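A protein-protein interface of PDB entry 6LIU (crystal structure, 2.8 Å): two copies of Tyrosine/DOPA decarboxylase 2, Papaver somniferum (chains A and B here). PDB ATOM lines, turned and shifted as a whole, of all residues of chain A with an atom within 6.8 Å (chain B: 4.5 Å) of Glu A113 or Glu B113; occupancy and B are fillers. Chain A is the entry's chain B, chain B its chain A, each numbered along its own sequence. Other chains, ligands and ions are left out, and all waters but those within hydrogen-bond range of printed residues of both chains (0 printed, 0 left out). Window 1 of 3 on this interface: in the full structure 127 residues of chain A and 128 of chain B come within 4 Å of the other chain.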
ATOM      1  N   LEU A  38     -12.655  -5.817  26.683  1.00  0.00           N
ATOM      2  CA  LEU A  38     -12.654  -6.389  28.027  1.00  0.00           C
ATOM      3  C   LEU A  38     -12.384  -5.327  29.087  1.00  0.00           C
ATOM      4  O   LEU A  38     -12.999  -5.343  30.162  1.00  0.00           O
ATOM      5  CB  LEU A  38     -11.625  -7.516  28.116  1.00  0.00           C
ATOM      6  CG  LEU A  38     -12.118  -8.851  27.549  1.00  0.00           C
ATOM      7  CD1 LEU A  38     -11.020  -9.905  27.571  1.00  0.00           C
ATOM      8  CD2 LEU A  38     -13.343  -9.320  28.318  1.00  0.00           C
ATOM      9  N   ALA A 108      -2.886  -9.907  36.359  1.00  0.00           N
ATOM     10  CA  ALA A 108      -1.724 -10.782  36.231  1.00  0.00           C
ATOM     11  C   ALA A 108      -2.133 -12.182  35.787  1.00  0.00           C
ATOM     12  O   ALA A 108      -1.521 -12.762  34.880  1.00  0.00           O
ATOM     13  CB  ALA A 108      -0.961 -10.833  37.555  1.00  0.00           C
ATOM     14  N   GLY A 109      -3.174 -12.738  36.412  1.00  0.00           N
ATOM     15  CA  GLY A 109      -3.631 -14.063  36.029  1.00  0.00           C
ATOM     16  C   GLY A 109      -4.147 -14.110  34.606  1.00  0.00           C
ATOM     17  O   GLY A 109      -3.894 -15.071  33.876  1.00  0.00           O
ATOM     18  N   PHE A 110      -4.886 -13.076  34.196  1.00  0.00           N
ATOM     19  CA  PHE A 110      -5.370 -13.006  32.822  1.00  0.00           C
ATOM     20  C   PHE A 110      -4.210 -13.011  31.834  1.00  0.00           C
ATOM     21  O   PHE A 110      -4.280 -13.668  30.787  1.00  0.00           O
ATOM     22  CB  PHE A 110      -6.240 -11.757  32.639  1.00  0.00           C
ATOM     23  CG  PHE A 110      -6.695 -11.523  31.217  1.00  0.00           C
ATOM     24  CD1 PHE A 110      -5.898 -10.827  30.316  1.00  0.00           C
ATOM     25  CD2 PHE A 110      -7.931 -11.981  30.789  1.00  0.00           C
ATOM     26  CE1 PHE A 110      -6.318 -10.609  29.015  1.00  0.00           C
ATOM     27  CE2 PHE A 110      -8.356 -11.764  29.488  1.00  0.00           C
ATOM     28  CZ  PHE A 110      -7.546 -11.076  28.603  1.00  0.00           C
ATOM     29  N   LEU A 111      -3.137 -12.279  32.145  1.00  0.00           N
ATOM     30  CA  LEU A 111      -1.986 -12.244  31.247  1.00  0.00           C
ATOM     31  C   LEU A 111      -1.300 -13.601  31.184  1.00  0.00           C
ATOM     32  O   LEU A 111      -0.861 -14.032  30.110  1.00  0.00           O
ATOM     33  CB  LEU A 111      -0.998 -11.163  31.690  1.00  0.00           C
ATOM     34  CG  LEU A 111      -1.516  -9.741  31.942  1.00  0.00           C
ATOM     35  CD1 LEU A 111      -0.395  -8.835  32.436  1.00  0.00           C
ATOM     36  CD2 LEU A 111      -2.183  -9.151  30.706  1.00  0.00           C
ATOM     37  N   GLY A 112      -1.207 -14.292  32.322  1.00  0.00           N
ATOM     38  CA  GLY A 112      -0.581 -15.605  32.332  1.00  0.00           C
ATOM     39  C   GLY A 112      -1.304 -16.610  31.458  1.00  0.00           C
ATOM     40  O   GLY A 112      -0.674 -17.418  30.769  1.00  0.00           O
ATOM     41  N   GLU A 113      -2.637 -16.581  31.473  1.00  0.00           N
ATOM     42  CA  GLU A 113      -3.380 -17.490  30.611  1.00  0.00           C
ATOM     43  C   GLU A 113      -3.295 -17.064  29.152  1.00  0.00           C
ATOM     44  O   GLU A 113      -3.418 -17.904  28.256  1.00  0.00           O
ATOM     45  CB  GLU A 113      -4.837 -17.581  31.061  1.00  0.00           C
ATOM     46  CG  GLU A 113      -5.214 -18.932  31.677  1.00  0.00           C
ATOM     47  CD  GLU A 113      -4.930 -20.115  30.758  1.00  0.00           C
ATOM     48  OE1 GLU A 113      -4.037 -20.936  31.079  1.00  0.00           O
ATOM     49  OE2 GLU A 113      -5.608 -20.227  29.715  1.00  0.00           O
ATOM     50  N   MET A 114      -3.085 -15.773  28.891  1.00  0.00           N
ATOM     51  CA  MET A 114      -2.940 -15.329  27.510  1.00  0.00           C
ATOM     52  C   MET A 114      -1.573 -15.696  26.954  1.00  0.00           C
ATOM     53  O   MET A 114      -1.460 -16.085  25.787  1.00  0.00           O
ATOM     54  CB  MET A 114      -3.190 -13.824  27.410  1.00  0.00           C
ATOM     55  CG  MET A 114      -4.676 -13.454  27.495  1.00  0.00           C
ATOM     56  SD  MET A 114      -5.761 -14.449  26.429  1.00  0.00           S
ATOM     57  CE  MET A 114      -6.466 -15.609  27.605  1.00  0.00           C
ATOM     58  N   LEU A 115      -0.527 -15.587  27.773  1.00  0.00           N
ATOM     59  CA  LEU A 115       0.764 -16.134  27.372  1.00  0.00           C
ATOM     60  C   LEU A 115       0.669 -17.639  27.161  1.00  0.00           C
ATOM     61  O   LEU A 115       1.245 -18.181  26.210  1.00  0.00           O
ATOM     62  CB  LEU A 115       1.827 -15.798  28.418  1.00  0.00           C
ATOM     63  CG  LEU A 115       2.325 -14.353  28.391  1.00  0.00           C
ATOM     64  CD1 LEU A 115       3.247 -14.084  29.566  1.00  0.00           C
ATOM     65  CD2 LEU A 115       3.025 -14.070  27.073  1.00  0.00           C
ATOM     66  N   SER A 116      -0.067 -18.328  28.037  1.00  0.00           N
ATOM     67  CA  SER A 116      -0.288 -19.761  27.867  1.00  0.00           C
ATOM     68  C   SER A 116      -1.020 -20.056  26.562  1.00  0.00           C
ATOM     69  O   SER A 116      -0.565 -20.872  25.753  1.00  0.00           O
ATOM     70  CB  SER A 116      -1.074 -20.304  29.061  1.00  0.00           C
ATOM     71  OG  SER A 116      -0.793 -21.672  29.283  1.00  0.00           O
ATOM     72  N   THR A 117      -2.164 -19.400  26.344  1.00  0.00           N
ATOM     73  CA  THR A 117      -2.900 -19.559  25.094  1.00  0.00           C
ATOM     74  C   THR A 117      -2.085 -19.084  23.898  1.00  0.00           C
ATOM     75  O   THR A 117      -2.255 -19.600  22.786  1.00  0.00           O
ATOM     76  CB  THR A 117      -4.223 -18.795  25.170  1.00  0.00           C
ATOM     77  OG1 THR A 117      -4.944 -19.202  26.339  1.00  0.00           O
ATOM     78  CG2 THR A 117      -5.079 -19.054  23.937  1.00  0.00           C
ATOM     79  N   GLY A 118      -1.199 -18.107  24.106  1.00  0.00           N
ATOM     80  CA  GLY A 118      -0.384 -17.615  23.006  1.00  0.00           C
ATOM     81  C   GLY A 118       0.678 -18.612  22.581  1.00  0.00           C
ATOM     82  O   GLY A 118       0.892 -18.841  21.387  1.00  0.00           O
ATOM     83  N   THR A 324      -6.801 -16.877  37.144  1.00  0.00           N
ATOM     84  CA  THR A 324      -8.036 -17.083  36.409  1.00  0.00           C
ATOM     85  C   THR A 324      -8.496 -18.538  36.543  1.00  0.00           C
ATOM     86  O   THR A 324      -7.699 -19.439  36.820  1.00  0.00           O
ATOM     87  CB  THR A 324      -7.818 -16.674  34.952  1.00  0.00           C
ATOM     88  OG1 THR A 324      -7.950 -15.251  34.849  1.00  0.00           O
ATOM     89  CG2 THR A 324      -8.802 -17.335  34.012  1.00  0.00           C
ATOM     90  N   LEU A 325      -9.809 -18.747  36.420  1.00  0.00           N
ATOM     91  CA  LEU A 325     -10.356 -20.085  36.202  1.00  0.00           C
ATOM     92  C   LEU A 325      -9.696 -20.753  34.998  1.00  0.00           C
ATOM     93  O   LEU A 325      -9.721 -20.214  33.890  1.00  0.00           O
ATOM     94  CB  LEU A 325     -11.865 -19.978  35.969  1.00  0.00           C
ATOM     95  CG  LEU A 325     -12.690 -21.236  35.713  1.00  0.00           C
ATOM     96  CD1 LEU A 325     -12.915 -21.969  37.014  1.00  0.00           C
ATOM     97  CD2 LEU A 325     -14.009 -20.863  35.066  1.00  0.00           C
ATOM     98  N   ASP A 326      -9.118 -21.934  35.192  1.00  0.00           N
ATOM     99  CA  ASP A 326      -9.150 -22.694  36.430  1.00  0.00           C
ATOM    100  C   ASP A 326      -7.722 -23.129  36.788  1.00  0.00           C
ATOM    101  O   ASP A 326      -6.888 -23.300  35.907  1.00  0.00           O
ATOM    102  CB  ASP A 326     -10.035 -23.930  36.282  1.00  0.00           C
ATOM    103  CG  ASP A 326      -9.649 -24.789  35.078  1.00  0.00           C
ATOM    104  OD1 ASP A 326      -8.820 -24.338  34.247  1.00  0.00           O
ATOM    105  OD2 ASP A 326     -10.148 -25.927  34.960  1.00  0.00           O
ATOM    106  N   ARG A 372      -2.164 -28.184  30.123  1.00  0.00           N
ATOM    107  CA  ARG A 372      -2.068 -26.762  29.837  1.00  0.00           C
ATOM    108  C   ARG A 372      -1.017 -26.114  30.731  1.00  0.00           C
ATOM    109  O   ARG A 372      -0.780 -26.542  31.864  1.00  0.00           O
ATOM    110  CB  ARG A 372      -3.419 -26.072  30.023  1.00  0.00           C
ATOM    111  CG  ARG A 372      -4.388 -26.321  28.883  1.00  0.00           C
ATOM    112  CD  ARG A 372      -5.639 -25.479  29.027  1.00  0.00           C
ATOM    113  NE  ARG A 372      -5.416 -24.103  28.598  1.00  0.00           N
ATOM    114  CZ  ARG A 372      -6.378 -23.193  28.475  1.00  0.00           C
ATOM    115  NH1 ARG A 372      -7.638 -23.509  28.748  1.00  0.00           N
ATOM    116  NH2 ARG A 372      -6.079 -21.966  28.074  1.00  0.00           N
ATOM    117  N   PHE A 373      -0.384 -25.071  30.193  1.00  0.00           N
ATOM    118  CA  PHE A 373       0.694 -24.340  30.861  1.00  0.00           C
ATOM    119  C   PHE A 373       0.085 -23.407  31.912  1.00  0.00           C
ATOM    120  O   PHE A 373       0.131 -22.179  31.818  1.00  0.00           O
ATOM    121  CB  PHE A 373       1.509 -23.592  29.813  1.00  0.00           C
ATOM    122  CG  PHE A 373       2.873 -23.149  30.265  1.00  0.00           C
ATOM    123  CD1 PHE A 373       3.232 -23.136  31.604  1.00  0.00           C
ATOM    124  CD2 PHE A 373       3.798 -22.724  29.327  1.00  0.00           C
ATOM    125  CE1 PHE A 373       4.495 -22.713  31.994  1.00  0.00           C
ATOM    126  CE2 PHE A 373       5.053 -22.301  29.711  1.00  0.00           C
ATOM    127  CZ  PHE A 373       5.404 -22.297  31.046  1.00  0.00           C
ATOM    128  N   ARG A 374      -0.489 -24.027  32.948  1.00  0.00           N
ATOM    129  CA  ARG A 374      -1.181 -23.283  33.996  1.00  0.00           C
ATOM    130  C   ARG A 374      -0.233 -22.548  34.932  1.00  0.00           C
ATOM    131  O   ARG A 374      -0.672 -21.631  35.636  1.00  0.00           O
ATOM    132  CB  ARG A 374      -2.057 -24.223  34.823  1.00  0.00           C
ATOM    133  CG  ARG A 374      -3.405 -24.542  34.213  1.00  0.00           C
ATOM    134  CD  ARG A 374      -4.256 -25.313  35.200  1.00  0.00           C
ATOM    135  NE  ARG A 374      -5.589 -25.580  34.678  1.00  0.00           N
ATOM    136  CZ  ARG A 374      -5.953 -26.731  34.128  1.00  0.00           C
ATOM    137  NH1 ARG A 374      -5.082 -27.725  34.038  1.00  0.00           N
ATOM    138  NH2 ARG A 374      -7.188 -26.887  33.674  1.00  0.00           N
ATOM    139  N   SER A 375       1.044 -22.934  34.975  1.00  0.00           N
ATOM    140  CA  SER A 375       1.962 -22.332  35.933  1.00  0.00           C
ATOM    141  C   SER A 375       2.233 -20.863  35.640  1.00  0.00           C
ATOM    142  O   SER A 375       2.624 -20.126  36.553  1.00  0.00           O
ATOM    143  CB  SER A 375       3.272 -23.111  35.960  1.00  0.00           C
ATOM    144  OG  SER A 375       3.573 -23.618  34.676  1.00  0.00           O
ATOM    145  N   LEU A 376       2.037 -20.423  34.393  1.00  0.00           N
ATOM    146  CA  LEU A 376       2.196 -19.008  34.081  1.00  0.00           C
ATOM    147  C   LEU A 376       1.210 -18.159  34.875  1.00  0.00           C
ATOM    148  O   LEU A 376       1.578 -17.107  35.408  1.00  0.00           O
ATOM    149  CB  LEU A 376       2.023 -18.780  32.579  1.00  0.00           C
ATOM    150  CG  LEU A 376       3.085 -19.395  31.665  1.00  0.00           C
ATOM    151  CD1 LEU A 376       2.645 -19.343  30.209  1.00  0.00           C
ATOM    152  CD2 LEU A 376       4.425 -18.693  31.849  1.00  0.00           C
ATOM    153  N   LYS A 377      -0.046 -18.603  34.970  1.00  0.00           N
ATOM    154  CA  LYS A 377      -1.025 -17.921  35.811  1.00  0.00           C
ATOM    155  C   LYS A 377      -0.495 -17.730  37.225  1.00  0.00           C
ATOM    156  O   LYS A 377      -0.473 -16.613  37.755  1.00  0.00           O
ATOM    157  CB  LYS A 377      -2.328 -18.721  35.854  1.00  0.00           C
ATOM    158  CG  LYS A 377      -3.408 -18.264  34.903  1.00  0.00           C
ATOM    159  CD  LYS A 377      -4.699 -19.028  35.176  1.00  0.00           C
ATOM    160  CE  LYS A 377      -4.453 -20.528  35.201  1.00  0.00           C
ATOM    161  NZ  LYS A 377      -5.588 -21.289  34.600  1.00  0.00           N
ATOM    162  N   MET A 380       2.606 -15.420  37.359  1.00  0.00           N
ATOM    163  CA  MET A 380       2.282 -14.008  37.185  1.00  0.00           C
ATOM    164  C   MET A 380       1.710 -13.405  38.462  1.00  0.00           C
ATOM    165  O   MET A 380       2.086 -12.294  38.854  1.00  0.00           O
ATOM    166  CB  MET A 380       1.298 -13.830  36.031  1.00  0.00           C
ATOM    167  CG  MET A 380       1.850 -14.221  34.678  1.00  0.00           C
ATOM    168  SD  MET A 380       3.146 -13.118  34.118  1.00  0.00           S
ATOM    169  CE  MET A 380       2.240 -12.118  32.945  1.00  0.00           C
ATOM    170  N   GLY B 109      -9.636 -18.453  17.790  1.00  0.00           N
ATOM    171  CA  GLY B 109      -9.589 -19.258  19.000  1.00  0.00           C
ATOM    172  C   GLY B 109      -8.995 -18.498  20.169  1.00  0.00           C
ATOM    173  O   GLY B 109      -9.530 -18.521  21.281  1.00  0.00           O
ATOM    174  N   PHE B 110      -7.883 -17.803  19.927  1.00  0.00           N
ATOM    175  CA  PHE B 110      -7.252 -17.007  20.976  1.00  0.00           C
ATOM    176  C   PHE B 110      -8.226 -15.983  21.546  1.00  0.00           C
ATOM    177  O   PHE B 110      -8.346 -15.835  22.767  1.00  0.00           O
ATOM    178  CB  PHE B 110      -6.003 -16.319  20.422  1.00  0.00           C
ATOM    179  CG  PHE B 110      -5.259 -15.494  21.433  1.00  0.00           C
ATOM    180  CD1 PHE B 110      -5.585 -14.159  21.637  1.00  0.00           C
ATOM    181  CD2 PHE B 110      -4.221 -16.045  22.165  1.00  0.00           C
ATOM    182  CE1 PHE B 110      -4.900 -13.395  22.560  1.00  0.00           C
ATOM    183  CE2 PHE B 110      -3.525 -15.283  23.092  1.00  0.00           C
ATOM    184  CZ  PHE B 110      -3.866 -13.957  23.290  1.00  0.00           C
ATOM    185  N   LEU B 111      -8.932 -15.264  20.674  1.00  0.00           N
ATOM    186  CA  LEU B 111      -9.870 -14.256  21.151  1.00  0.00           C
ATOM    187  C   LEU B 111     -11.023 -14.878  21.926  1.00  0.00           C
ATOM    188  O   LEU B 111     -11.568 -14.242  22.834  1.00  0.00           O
ATOM    189  CB  LEU B 111     -10.394 -13.436  19.976  1.00  0.00           C
ATOM    190  CG  LEU B 111      -9.308 -12.733  19.159  1.00  0.00           C
ATOM    191  CD1 LEU B 111      -9.926 -11.898  18.049  1.00  0.00           C
ATOM    192  CD2 LEU B 111      -8.401 -11.884  20.054  1.00  0.00           C
ATOM    193  N   GLY B 112     -11.407 -16.110  21.581  1.00  0.00           N
ATOM    194  CA  GLY B 112     -12.449 -16.787  22.336  1.00  0.00           C
ATOM    195  C   GLY B 112     -12.008 -17.119  23.750  1.00  0.00           C
ATOM    196  O   GLY B 112     -12.747 -16.898  24.715  1.00  0.00           O
ATOM    197  N   GLU B 113     -10.793 -17.657  23.891  1.00  0.00           N
ATOM    198  CA  GLU B 113     -10.245 -17.895  25.222  1.00  0.00           C
ATOM    199  C   GLU B 113     -10.010 -16.590  25.968  1.00  0.00           C
ATOM    200  O   GLU B 113     -10.157 -16.538  27.193  1.00  0.00           O
ATOM    201  CB  GLU B 113      -8.940 -18.687  25.124  1.00  0.00           C
ATOM    202  CG  GLU B 113      -9.061 -20.146  25.535  1.00  0.00           C
ATOM    203  CD  GLU B 113      -9.510 -20.318  26.971  1.00  0.00           C
ATOM    204  OE1 GLU B 113      -8.645 -20.285  27.870  1.00  0.00           O
ATOM    205  OE2 GLU B 113     -10.727 -20.489  27.200  1.00  0.00           O
ATOM    206  N   MET B 114      -9.642 -15.531  25.246  1.00  0.00           N
ATOM    207  CA  MET B 114      -9.478 -14.221  25.868  1.00  0.00           C
ATOM    208  C   MET B 114     -10.800 -13.719  26.440  1.00  0.00           C
ATOM    209  O   MET B 114     -10.856 -13.229  27.575  1.00  0.00           O
ATOM    210  CB  MET B 114      -8.919 -13.240  24.839  1.00  0.00           C
ATOM    211  CG  MET B 114      -8.188 -12.057  25.426  1.00  0.00           C
ATOM    212  SD  MET B 114      -7.213 -11.165  24.195  1.00  0.00           S
ATOM    213  CE  MET B 114      -5.661 -11.027  25.075  1.00  0.00           C
ATOM    214  N   LEU B 115     -11.882 -13.833  25.666  1.00  0.00           N
ATOM    215  CA  LEU B 115     -13.191 -13.435  26.167  1.00  0.00           C
ATOM    216  C   LEU B 115     -13.611 -14.306  27.343  1.00  0.00           C
ATOM    217  O   LEU B 115     -14.092 -13.802  28.366  1.00  0.00           O
ATOM    218  CB  LEU B 115     -14.227 -13.511  25.046  1.00  0.00           C
ATOM    219  CG  LEU B 115     -14.269 -12.349  24.054  1.00  0.00           C
ATOM    220  CD1 LEU B 115     -15.357 -12.572  23.017  1.00  0.00           C
ATOM    221  CD2 LEU B 115     -14.488 -11.039  24.787  1.00  0.00           C
ATOM    222  N   SER B 116     -13.436 -15.625  27.216  1.00  0.00           N
ATOM    223  CA  SER B 116     -13.800 -16.528  28.302  1.00  0.00           C
ATOM    224  C   SER B 116     -13.006 -16.208  29.562  1.00  0.00           C
ATOM    225  O   SER B 116     -13.577 -16.043  30.646  1.00  0.00           O
ATOM    226  CB  SER B 116     -13.576 -17.978  27.877  1.00  0.00           C
ATOM    227  OG  SER B 116     -13.213 -18.779  28.987  1.00  0.00           O
ATOM    228  N   THR B 117     -11.683 -16.113  29.432  1.00  0.00           N
ATOM    229  CA  THR B 117     -10.858 -15.696  30.558  1.00  0.00           C
ATOM    230  C   THR B 117     -11.267 -14.314  31.055  1.00  0.00           C
ATOM    231  O   THR B 117     -11.328 -14.074  32.268  1.00  0.00           O
ATOM    232  CB  THR B 117      -9.387 -15.710  30.150  1.00  0.00           C
ATOM    233  OG1 THR B 117      -9.031 -17.027  29.713  1.00  0.00           O
ATOM    234  CG2 THR B 117      -8.497 -15.305  31.307  1.00  0.00           C
ATOM    235  N   THR B 324      -7.746 -22.979  20.401  1.00  0.00           N
ATOM    236  CA  THR B 324      -6.541 -23.260  21.165  1.00  0.00           C
ATOM    237  C   THR B 324      -6.796 -24.392  22.163  1.00  0.00           C
ATOM    238  O   THR B 324      -7.930 -24.825  22.384  1.00  0.00           O
ATOM    239  CB  THR B 324      -6.064 -22.007  21.889  1.00  0.00           C
ATOM    240  OG1 THR B 324      -7.160 -21.426  22.608  1.00  0.00           O
ATOM    241  CG2 THR B 324      -5.526 -20.999  20.886  1.00  0.00           C
ATOM    242  N   ARG B 372     -15.474 -24.242  32.297  1.00  0.00           N
ATOM    243  CA  ARG B 372     -15.025 -23.040  31.615  1.00  0.00           C
ATOM    244  C   ARG B 372     -15.915 -22.752  30.407  1.00  0.00           C
ATOM    245  O   ARG B 372     -16.645 -23.617  29.916  1.00  0.00           O
ATOM    246  CB  ARG B 372     -13.562 -23.174  31.183  1.00  0.00           C
ATOM    247  CG  ARG B 372     -12.572 -22.987  32.329  1.00  0.00           C
ATOM    248  CD  ARG B 372     -11.128 -23.158  31.881  1.00  0.00           C
ATOM    249  NE  ARG B 372     -10.613 -21.961  31.222  1.00  0.00           N
ATOM    250  CZ  ARG B 372      -9.320 -21.694  31.056  1.00  0.00           C
ATOM    251  NH1 ARG B 372      -8.395 -22.534  31.505  1.00  0.00           N
ATOM    252  NH2 ARG B 372      -8.951 -20.581  30.441  1.00  0.00           N
ATOM    253  N   LYS B 377     -14.537 -20.058  22.206  1.00  0.00           N
ATOM    254  CA  LYS B 377     -13.517 -20.532  21.274  1.00  0.00           C
ATOM    255  C   LYS B 377     -14.140 -21.108  20.006  1.00  0.00           C
ATOM    256  O   LYS B 377     -13.865 -20.649  18.893  1.00  0.00           O
ATOM    257  CB  LYS B 377     -12.652 -21.598  21.952  1.00  0.00           C
ATOM    258  CG  LYS B 377     -11.642 -21.084  22.939  1.00  0.00           C
ATOM    259  CD  LYS B 377     -10.578 -22.144  23.179  1.00  0.00           C
ATOM    260  CE  LYS B 377     -11.130 -23.311  23.970  1.00  0.00           C
ATOM    261  NZ  LYS B 377     -10.115 -23.870  24.905  1.00  0.00           N
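The side-chain hydroxyl (OG1) of Thr B117 sits at hydrogen-bond distance from the backbone carbonyl oxygen (O) of Glu B113 (2.8 Å). OE2 of Glu A113 lies within salt-bridge range of NH2 of Arg A372, 2.4 Å away. OE1 of Glu A113 lies within salt-bridge range of NZ of Lys A377, at 3.9 Å. The backbone carbonyl oxygen of Glu A113 is in hydrogen-bond range of the side-chain hydroxyl of Thr A117, at 2.8 Å. The side-chain carboxylate of Glu B113 is in salt-bridge range of the guanidinium group of Arg B372, 2.6 Å away. The side-chain hydroxyl (OG1) of Thr A117 is in hydrogen-bond range of the guanidinium group (NH2) of Arg A372 (3.5 Å).
Among the printed residues, merely in contact across the chains: Leu A38 with Met B114, Phe A110 with Met B114, Phe A110 with Thr B117, Glu A113 with Glu B113, Met A114 with Phe B110, Met A114 with Glu B113, Met A114 with Met B114, Met A114 with Thr B117, Thr A117 with Phe B110, Thr A117 with Thr B324, Gly A118 with Phe B110 and Thr A324 with Thr B117.
Glu A113 touches its own counterpart, Glu B113. Met A114 touches Glu B113, but with the chains exchanged Glu A113 does not touch Met B114 (7.3 Å). Met A114 touches Thr B117, but with the chains exchanged Thr A117 does not touch Met B114 (5.9 Å). Arg B372 touches its own counterpart, Arg A372. Of the 17 pairs that touch across the chains among the printed residues, 11 have their exchanged pair printed and touching as well.
Printed residues of chain B within 4 Å of Leu A38: Met B114. Printed residues of chain B within 4 Å of Phe A110: Met B114 and Thr B117. Glu A113 touches two residues of chain B. Of the printed residues of chain B, Thr A117 touches Phe B110 and Thr B324. Of the printed residues of chain B, Gly A118 touches Phe B110. Printed residues of chain B within 4 Å of Leu A325: Arg B372. Leu A376 touches none of the printed residues of chain B. Glu B113 touches three residues of chain A. Ser B116 touches none of the printed residues of chain A. The nearest residue of chain B that does not touch Glu A113 is Thr B117 (4.3 Å). The nearest residue of chain A that does not touch Glu B113 is Thr A117 (4.1 Å).
NH1 of Arg B372 sits close to NH1 of Arg A372. O of Leu A325 lies close to NE of Arg B372 (3.3 Å). The side-chain carboxylate (OE1) of Glu B113 lies within salt-bridge range of the guanidinium group (NH2) of Arg A372 (3.1 Å). The guanidinium group (NH1) of Arg B372 lies within salt-bridge range of the side-chain carboxylate (OD1) of Asp A326, 3.3 Å away. OE2 of Glu A113 lies within salt-bridge range of NH2 of Arg B372 (3.4 Å).
Of the 22 printed residues of chain A, 10 touch a printed residue of chain B. Hydrophobic or aromatic side chains of chain A within 4 Å of the printed part of chain B: Leu A38, Phe A110, Met A114 and Leu A325. Along chain A the printed residues that touch a printed residue of chain B span positions 38 to 372. Among the printed residues, Asp or Glu carboxylates within 4 Å of a Lys or Arg side-chain nitrogen of the other chain: Glu A113 with Arg B372, Asp A326 with Arg B372 and Arg A372 with Glu B113.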
